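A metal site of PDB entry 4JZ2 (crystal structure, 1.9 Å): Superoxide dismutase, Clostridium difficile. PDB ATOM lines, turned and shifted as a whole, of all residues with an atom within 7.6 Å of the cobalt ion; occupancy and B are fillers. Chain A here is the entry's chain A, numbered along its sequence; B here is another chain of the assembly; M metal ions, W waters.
ND1 of His 34 lies close to ND1 of His 171 (3.5 Å). N of Trp 169 sits at hydrogen-bond distance from OD1 of Asp 167. A ring nitrogen (ND1) of His 171 lies within hydrogen-bond range of the side-chain carboxylate (OE2) of Glu 170 of chain B (2.7 Å). The backbone carbonyl oxygen of His 30 lies within hydrogen-bond range of the backbone NH of Tyr 35 (2.9 Å). The backbone carbonyl oxygen (O) of Asp 167 sits at hydrogen-bond distance from the side-chain hydroxyl (OH) of Tyr 184 (2.8 Å). ND1 of His 85 is in hydrogen-bond range of O of Gly 81.
The cobalt ion is bound by the side-chain carboxylate (OD2) of Asp 167 (2.0 Å), a ring nitrogen (NE2) of His 85 (2.1 Å), a ring nitrogen (NE2) of His 171 (2.2 Å), a ring nitrogen (NE2) of His 30 (2.2 Å) and water W1 (2.4 Å). The cobalt ion has five donor atoms within binding distance.
Water W1 lies within hydrogen-bond range of NE2 of Gln 152 (2.8 Å), OD1 of Asp 167 (2.8 Å) and NE1 of Trp 169 (3.4 Å).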
ATOM      1  N   HIS A  30       9.468  -8.611 -30.010  1.00  0.00           N
ATOM      2  CA  HIS A  30      10.641  -7.782 -29.768  1.00  0.00           C
ATOM      3  C   HIS A  30      10.258  -6.521 -29.013  1.00  0.00           C
ATOM      4  O   HIS A  30      10.887  -6.169 -28.009  1.00  0.00           O
ATOM      5  CB  HIS A  30      11.298  -7.427 -31.093  1.00  0.00           C
ATOM      6  CG  HIS A  30      12.767  -7.153 -30.980  1.00  0.00           C
ATOM      7  ND1 HIS A  30      13.520  -6.738 -32.064  1.00  0.00           N
ATOM      8  CD2 HIS A  30      13.620  -7.236 -29.937  1.00  0.00           C
ATOM      9  CE1 HIS A  30      14.765  -6.571 -31.685  1.00  0.00           C
ATOM     10  NE2 HIS A  30      14.858  -6.875 -30.394  1.00  0.00           N
ATOM     11  N   HIS A  31       9.209  -5.849 -29.486  1.00  0.00           N
ATOM     12  CA  HIS A  31       8.764  -4.601 -28.870  1.00  0.00           C
ATOM     13  C   HIS A  31       7.949  -4.824 -27.600  1.00  0.00           C
ATOM     14  O   HIS A  31       8.213  -4.224 -26.556  1.00  0.00           O
ATOM     15  CB  HIS A  31       7.934  -3.775 -29.876  1.00  0.00           C
ATOM     16  CG  HIS A  31       7.414  -2.492 -29.301  1.00  0.00           C
ATOM     17  ND1 HIS A  31       6.290  -2.433 -28.505  1.00  0.00           N
ATOM     18  CD2 HIS A  31       7.872  -1.222 -29.407  1.00  0.00           C
ATOM     19  CE1 HIS A  31       6.075  -1.178 -28.145  1.00  0.00           C
ATOM     20  NE2 HIS A  31       7.020  -0.425 -28.681  1.00  0.00           N
ATOM     21  N   HIS A  34      10.375  -8.148 -25.163  1.00  0.00           N
ATOM     22  CA  HIS A  34      11.781  -7.878 -24.844  1.00  0.00           C
ATOM     23  C   HIS A  34      12.033  -6.437 -24.425  1.00  0.00           C
ATOM     24  O   HIS A  34      12.600  -6.183 -23.357  1.00  0.00           O
ATOM     25  CB  HIS A  34      12.688  -8.245 -26.012  1.00  0.00           C
ATOM     26  CG  HIS A  34      12.707  -9.708 -26.331  1.00  0.00           C
ATOM     27  ND1 HIS A  34      13.580 -10.581 -25.716  1.00  0.00           N
ATOM     28  CD2 HIS A  34      11.968 -10.454 -27.188  1.00  0.00           C
ATOM     29  CE1 HIS A  34      13.371 -11.801 -26.185  1.00  0.00           C
ATOM     30  NE2 HIS A  34      12.398 -11.744 -27.082  1.00  0.00           N
ATOM     31  N   TYR A  35      11.611  -5.484 -25.242  1.00  0.00           N
ATOM     32  CA  TYR A  35      11.834  -4.075 -24.945  1.00  0.00           C
ATOM     33  C   TYR A  35      11.100  -3.715 -23.659  1.00  0.00           C
ATOM     34  O   TYR A  35      11.675  -3.108 -22.735  1.00  0.00           O
ATOM     35  CB  TYR A  35      11.376  -3.235 -26.146  1.00  0.00           C
ATOM     36  CG  TYR A  35      11.395  -1.718 -25.985  1.00  0.00           C
ATOM     37  CD1 TYR A  35      12.213  -1.079 -25.043  1.00  0.00           C
ATOM     38  CD2 TYR A  35      10.616  -0.923 -26.826  1.00  0.00           C
ATOM     39  CE1 TYR A  35      12.213   0.320 -24.924  1.00  0.00           C
ATOM     40  CE2 TYR A  35      10.607   0.450 -26.719  1.00  0.00           C
ATOM     41  CZ  TYR A  35      11.398   1.075 -25.777  1.00  0.00           C
ATOM     42  OH  TYR A  35      11.354   2.450 -25.718  1.00  0.00           O
ATOM     43  N   TYR A  38      12.992  -4.828 -20.446  1.00  0.00           N
ATOM     44  CA  TYR A  38      14.115  -3.965 -20.065  1.00  0.00           C
ATOM     45  C   TYR A  38      13.602  -2.735 -19.326  1.00  0.00           C
ATOM     46  O   TYR A  38      14.164  -2.340 -18.313  1.00  0.00           O
ATOM     47  CB  TYR A  38      14.931  -3.544 -21.284  1.00  0.00           C
ATOM     48  CG  TYR A  38      15.673  -4.692 -21.930  1.00  0.00           C
ATOM     49  CD1 TYR A  38      16.578  -5.451 -21.204  1.00  0.00           C
ATOM     50  CD2 TYR A  38      15.470  -5.005 -23.260  1.00  0.00           C
ATOM     51  CE1 TYR A  38      17.273  -6.506 -21.796  1.00  0.00           C
ATOM     52  CE2 TYR A  38      16.142  -6.060 -23.860  1.00  0.00           C
ATOM     53  CZ  TYR A  38      17.039  -6.802 -23.122  1.00  0.00           C
ATOM     54  OH  TYR A  38      17.714  -7.841 -23.742  1.00  0.00           O
ATOM     55  N   GLY A  81      19.300  -1.943 -22.582  1.00  0.00           N
ATOM     56  CA  GLY A  81      18.243  -2.593 -23.357  1.00  0.00           C
ATOM     57  C   GLY A  81      17.157  -1.609 -23.765  1.00  0.00           C
ATOM     58  O   GLY A  81      16.694  -1.607 -24.903  1.00  0.00           O
ATOM     59  N   ASN A  84      18.761   0.964 -26.368  1.00  0.00           N
ATOM     60  CA  ASN A  84      19.131   0.349 -27.647  1.00  0.00           C
ATOM     61  C   ASN A  84      17.897  -0.023 -28.462  1.00  0.00           C
ATOM     62  O   ASN A  84      17.901   0.094 -29.679  1.00  0.00           O
ATOM     63  CB  ASN A  84      19.975  -0.913 -27.435  1.00  0.00           C
ATOM     64  CG  ASN A  84      21.345  -0.611 -26.838  1.00  0.00           C
ATOM     65  OD1 ASN A  84      21.804   0.527 -26.888  1.00  0.00           O
ATOM     66  ND2 ASN A  84      21.993  -1.638 -26.275  1.00  0.00           N
ATOM     67  N   HIS A  85      16.844  -0.478 -27.786  1.00  0.00           N
ATOM     68  CA  HIS A  85      15.661  -0.904 -28.509  1.00  0.00           C
ATOM     69  C   HIS A  85      14.832   0.279 -28.992  1.00  0.00           C
ATOM     70  O   HIS A  85      14.334   0.283 -30.118  1.00  0.00           O
ATOM     71  CB  HIS A  85      14.833  -1.899 -27.683  1.00  0.00           C
ATOM     72  CG  HIS A  85      15.444  -3.259 -27.627  1.00  0.00           C
ATOM     73  ND1 HIS A  85      16.402  -3.613 -26.690  1.00  0.00           N
ATOM     74  CD2 HIS A  85      15.291  -4.334 -28.437  1.00  0.00           C
ATOM     75  CE1 HIS A  85      16.783  -4.859 -26.909  1.00  0.00           C
ATOM     76  NE2 HIS A  85      16.130  -5.318 -27.963  1.00  0.00           N
ATOM     77  N   PHE A  88      16.646   1.281 -31.908  1.00  0.00           N
ATOM     78  CA  PHE A  88      16.559   0.313 -32.994  1.00  0.00           C
ATOM     79  C   PHE A  88      15.234   0.422 -33.771  1.00  0.00           C
ATOM     80  O   PHE A  88      15.225   0.455 -35.007  1.00  0.00           O
ATOM     81  CB  PHE A  88      16.742  -1.100 -32.431  1.00  0.00           C
ATOM     82  CG  PHE A  88      16.740  -2.189 -33.474  1.00  0.00           C
ATOM     83  CD1 PHE A  88      17.659  -2.183 -34.502  1.00  0.00           C
ATOM     84  CD2 PHE A  88      15.852  -3.259 -33.379  1.00  0.00           C
ATOM     85  CE1 PHE A  88      17.661  -3.191 -35.467  1.00  0.00           C
ATOM     86  CE2 PHE A  88      15.856  -4.268 -34.323  1.00  0.00           C
ATOM     87  CZ  PHE A  88      16.751  -4.239 -35.367  1.00  0.00           C
ATOM     88  N   PHE A  89      14.123   0.498 -33.054  1.00  0.00           N
ATOM     89  CA  PHE A  89      12.831   0.611 -33.743  1.00  0.00           C
ATOM     90  C   PHE A  89      12.733   1.964 -34.458  1.00  0.00           C
ATOM     91  O   PHE A  89      12.142   2.062 -35.538  1.00  0.00           O
ATOM     92  CB  PHE A  89      11.677   0.382 -32.784  1.00  0.00           C
ATOM     93  CG  PHE A  89      11.705  -0.968 -32.113  1.00  0.00           C
ATOM     94  CD1 PHE A  89      11.875  -2.122 -32.873  1.00  0.00           C
ATOM     95  CD2 PHE A  89      11.575  -1.079 -30.746  1.00  0.00           C
ATOM     96  CE1 PHE A  89      11.914  -3.364 -32.272  1.00  0.00           C
ATOM     97  CE2 PHE A  89      11.620  -2.333 -30.127  1.00  0.00           C
ATOM     98  CZ  PHE A  89      11.781  -3.469 -30.884  1.00  0.00           C
ATOM     99  N   GLY A 132      24.579  -9.272 -29.086  1.00  0.00           N
ATOM    100  CA  GLY A 132      25.136  -7.931 -29.171  1.00  0.00           C
ATOM    101  C   GLY A 132      24.618  -7.105 -30.329  1.00  0.00           C
ATOM    102  O   GLY A 132      23.573  -7.426 -30.899  1.00  0.00           O
ATOM    103  N   TRP A 133      25.368  -6.079 -30.692  1.00  0.00           N
ATOM    104  CA  TRP A 133      24.920  -5.055 -31.642  1.00  0.00           C
ATOM    105  C   TRP A 133      26.070  -4.643 -32.541  1.00  0.00           C
ATOM    106  O   TRP A 133      27.236  -4.669 -32.127  1.00  0.00           O
ATOM    107  CB  TRP A 133      24.452  -3.803 -30.892  1.00  0.00           C
ATOM    108  CG  TRP A 133      23.249  -4.006 -30.058  1.00  0.00           C
ATOM    109  CD1 TRP A 133      23.190  -4.606 -28.828  1.00  0.00           C
ATOM    110  CD2 TRP A 133      21.919  -3.593 -30.359  1.00  0.00           C
ATOM    111  NE1 TRP A 133      21.903  -4.609 -28.350  1.00  0.00           N
ATOM    112  CE2 TRP A 133      21.090  -3.990 -29.279  1.00  0.00           C
ATOM    113  CE3 TRP A 133      21.329  -2.928 -31.439  1.00  0.00           C
ATOM    114  CZ2 TRP A 133      19.721  -3.735 -29.241  1.00  0.00           C
ATOM    115  CZ3 TRP A 133      19.964  -2.681 -31.412  1.00  0.00           C
ATOM    116  CH2 TRP A 133      19.172  -3.084 -30.315  1.00  0.00           C
ATOM    117  N   GLN A 152      23.772  -5.739 -23.969  1.00  0.00           N
ATOM    118  CA  GLN A 152      23.099  -4.438 -24.158  1.00  0.00           C
ATOM    119  C   GLN A 152      24.036  -3.258 -23.893  1.00  0.00           C
ATOM    120  O   GLN A 152      23.581  -2.151 -23.593  1.00  0.00           O
ATOM    121  CB  GLN A 152      21.850  -4.331 -23.278  1.00  0.00           C
ATOM    122  CG  GLN A 152      20.727  -5.345 -23.634  1.00  0.00           C
ATOM    123  CD  GLN A 152      20.251  -5.261 -25.085  1.00  0.00           C
ATOM    124  OE1 GLN A 152      20.531  -4.293 -25.787  1.00  0.00           O
ATOM    125  NE2 GLN A 152      19.529  -6.294 -25.531  1.00  0.00           N
ATOM    126  N   ASP A 167      20.505  -4.859 -34.090  1.00  0.00           N
ATOM    127  CA  ASP A 167      20.378  -5.855 -33.029  1.00  0.00           C
ATOM    128  C   ASP A 167      20.693  -7.243 -33.611  1.00  0.00           C
ATOM    129  O   ASP A 167      19.978  -7.710 -34.511  1.00  0.00           O
ATOM    130  CB  ASP A 167      18.946  -5.816 -32.496  1.00  0.00           C
ATOM    131  CG  ASP A 167      18.734  -6.644 -31.250  1.00  0.00           C
ATOM    132  OD1 ASP A 167      19.671  -7.317 -30.780  1.00  0.00           O
ATOM    133  OD2 ASP A 167      17.590  -6.616 -30.718  1.00  0.00           O
ATOM    134  N   VAL A 168      21.755  -7.897 -33.137  1.00  0.00           N
ATOM    135  CA  VAL A 168      22.029  -9.268 -33.583  1.00  0.00           C
ATOM    136  C   VAL A 168      21.897 -10.319 -32.478  1.00  0.00           C
ATOM    137  O   VAL A 168      22.435 -11.432 -32.592  1.00  0.00           O
ATOM    138  CB  VAL A 168      23.362  -9.449 -34.356  1.00  0.00           C
ATOM    139  CG1 VAL A 168      23.315  -8.665 -35.670  1.00  0.00           C
ATOM    140  CG2 VAL A 168      24.555  -9.037 -33.494  1.00  0.00           C
ATOM    141  N   TRP A 169      21.185  -9.962 -31.415  1.00  0.00           N
ATOM    142  CA  TRP A 169      20.681 -10.974 -30.492  1.00  0.00           C
ATOM    143  C   TRP A 169      19.855 -11.923 -31.355  1.00  0.00           C
ATOM    144  O   TRP A 169      19.179 -11.481 -32.291  1.00  0.00           O
ATOM    145  CB  TRP A 169      19.780 -10.337 -29.457  1.00  0.00           C
ATOM    146  CG  TRP A 169      20.505  -9.624 -28.330  1.00  0.00           C
ATOM    147  CD1 TRP A 169      21.415  -8.597 -28.442  1.00  0.00           C
ATOM    148  CD2 TRP A 169      20.380  -9.897 -26.930  1.00  0.00           C
ATOM    149  NE1 TRP A 169      21.848  -8.211 -27.190  1.00  0.00           N
ATOM    150  CE2 TRP A 169      21.227  -8.992 -26.244  1.00  0.00           C
ATOM    151  CE3 TRP A 169      19.622 -10.811 -26.181  1.00  0.00           C
ATOM    152  CZ2 TRP A 169      21.344  -8.993 -24.851  1.00  0.00           C
ATOM    153  CZ3 TRP A 169      19.734 -10.802 -24.797  1.00  0.00           C
ATOM    154  CH2 TRP A 169      20.591  -9.897 -24.152  1.00  0.00           C
ATOM    155  N   GLU A 170      19.886 -13.220 -31.042  1.00  0.00           N
ATOM    156  CA  GLU A 170      19.120 -14.195 -31.821  1.00  0.00           C
ATOM    157  C   GLU A 170      17.605 -13.939 -31.764  1.00  0.00           C
ATOM    158  O   GLU A 170      16.886 -14.289 -32.701  1.00  0.00           O
ATOM    159  CB  GLU A 170      19.470 -15.629 -31.382  1.00  0.00           C
ATOM    160  CG  GLU A 170      20.900 -16.011 -31.820  1.00  0.00           C
ATOM    161  CD  GLU A 170      21.425 -17.323 -31.209  1.00  0.00           C
ATOM    162  OE1 GLU A 170      21.106 -17.640 -30.043  1.00  0.00           O
ATOM    163  OE2 GLU A 170      22.192 -18.020 -31.909  1.00  0.00           O
ATOM    164  N   HIS A 171      17.106 -13.340 -30.679  1.00  0.00           N
ATOM    165  CA  HIS A 171      15.673 -13.048 -30.654  1.00  0.00           C
ATOM    166  C   HIS A 171      15.219 -12.082 -31.770  1.00  0.00           C
ATOM    167  O   HIS A 171      14.047 -12.063 -32.154  1.00  0.00           O
ATOM    168  CB  HIS A 171      15.199 -12.578 -29.282  1.00  0.00           C
ATOM    169  CG  HIS A 171      15.740 -11.238 -28.862  1.00  0.00           C
ATOM    170  ND1 HIS A 171      16.414 -11.059 -27.678  1.00  0.00           N
ATOM    171  CD2 HIS A 171      15.670 -10.024 -29.453  1.00  0.00           C
ATOM    172  CE1 HIS A 171      16.761  -9.786 -27.565  1.00  0.00           C
ATOM    173  NE2 HIS A 171      16.310  -9.132 -28.624  1.00  0.00           N
ATOM    174  N   ALA A 172      16.152 -11.283 -32.270  1.00  0.00           N
ATOM    175  CA  ALA A 172      15.854 -10.313 -33.326  1.00  0.00           C
ATOM    176  C   ALA A 172      15.632 -10.960 -34.691  1.00  0.00           C
ATOM    177  O   ALA A 172      15.045 -10.342 -35.584  1.00  0.00           O
ATOM    178  CB  ALA A 172      16.987  -9.282 -33.453  1.00  0.00           C
ATOM    179  N   TYR A 184      19.586 -12.187 -42.522  1.00  0.00           N
ATOM    180  CA  TYR A 184      18.941 -11.158 -41.724  1.00  0.00           C
ATOM    181  C   TYR A 184      19.615  -9.809 -41.927  1.00  0.00           C
ATOM    182  O   TYR A 184      18.969  -8.800 -42.200  1.00  0.00           O
ATOM    183  CB  TYR A 184      19.014 -11.553 -40.260  1.00  0.00           C
ATOM    184  CG  TYR A 184      18.674 -10.478 -39.245  1.00  0.00           C
ATOM    185  CD1 TYR A 184      17.424  -9.864 -39.228  1.00  0.00           C
ATOM    186  CD2 TYR A 184      19.606 -10.126 -38.262  1.00  0.00           C
ATOM    187  CE1 TYR A 184      17.113  -8.890 -38.267  1.00  0.00           C
ATOM    188  CE2 TYR A 184      19.308  -9.177 -37.314  1.00  0.00           C
ATOM    189  CZ  TYR A 184      18.067  -8.559 -37.307  1.00  0.00           C
ATOM    190  OH  TYR A 184      17.811  -7.626 -36.334  1.00  0.00           O
ATOM    191  N   GLU B 170      19.513 -18.020 -27.045  1.00  0.00           N
ATOM    192  CA  GLU B 170      18.147 -17.957 -27.562  1.00  0.00           C
ATOM    193  C   GLU B 170      17.892 -18.971 -28.692  1.00  0.00           C
ATOM    194  O   GLU B 170      16.766 -19.409 -28.886  1.00  0.00           O
ATOM    195  CB  GLU B 170      17.793 -16.514 -28.000  1.00  0.00           C
ATOM    196  CG  GLU B 170      17.656 -15.589 -26.783  1.00  0.00           C
ATOM    197  CD  GLU B 170      17.558 -14.096 -27.121  1.00  0.00           C
ATOM    198  OE1 GLU B 170      18.210 -13.635 -28.092  1.00  0.00           O
ATOM    199  OE2 GLU B 170      16.854 -13.370 -26.392  1.00  0.00           O
HETATM  200 CO    CO M   1      16.568  -7.043 -29.083  1.00  0.00          CO
HETATM  201  O   HOH W   1      18.770  -7.103 -28.107  1.00  0.00           O
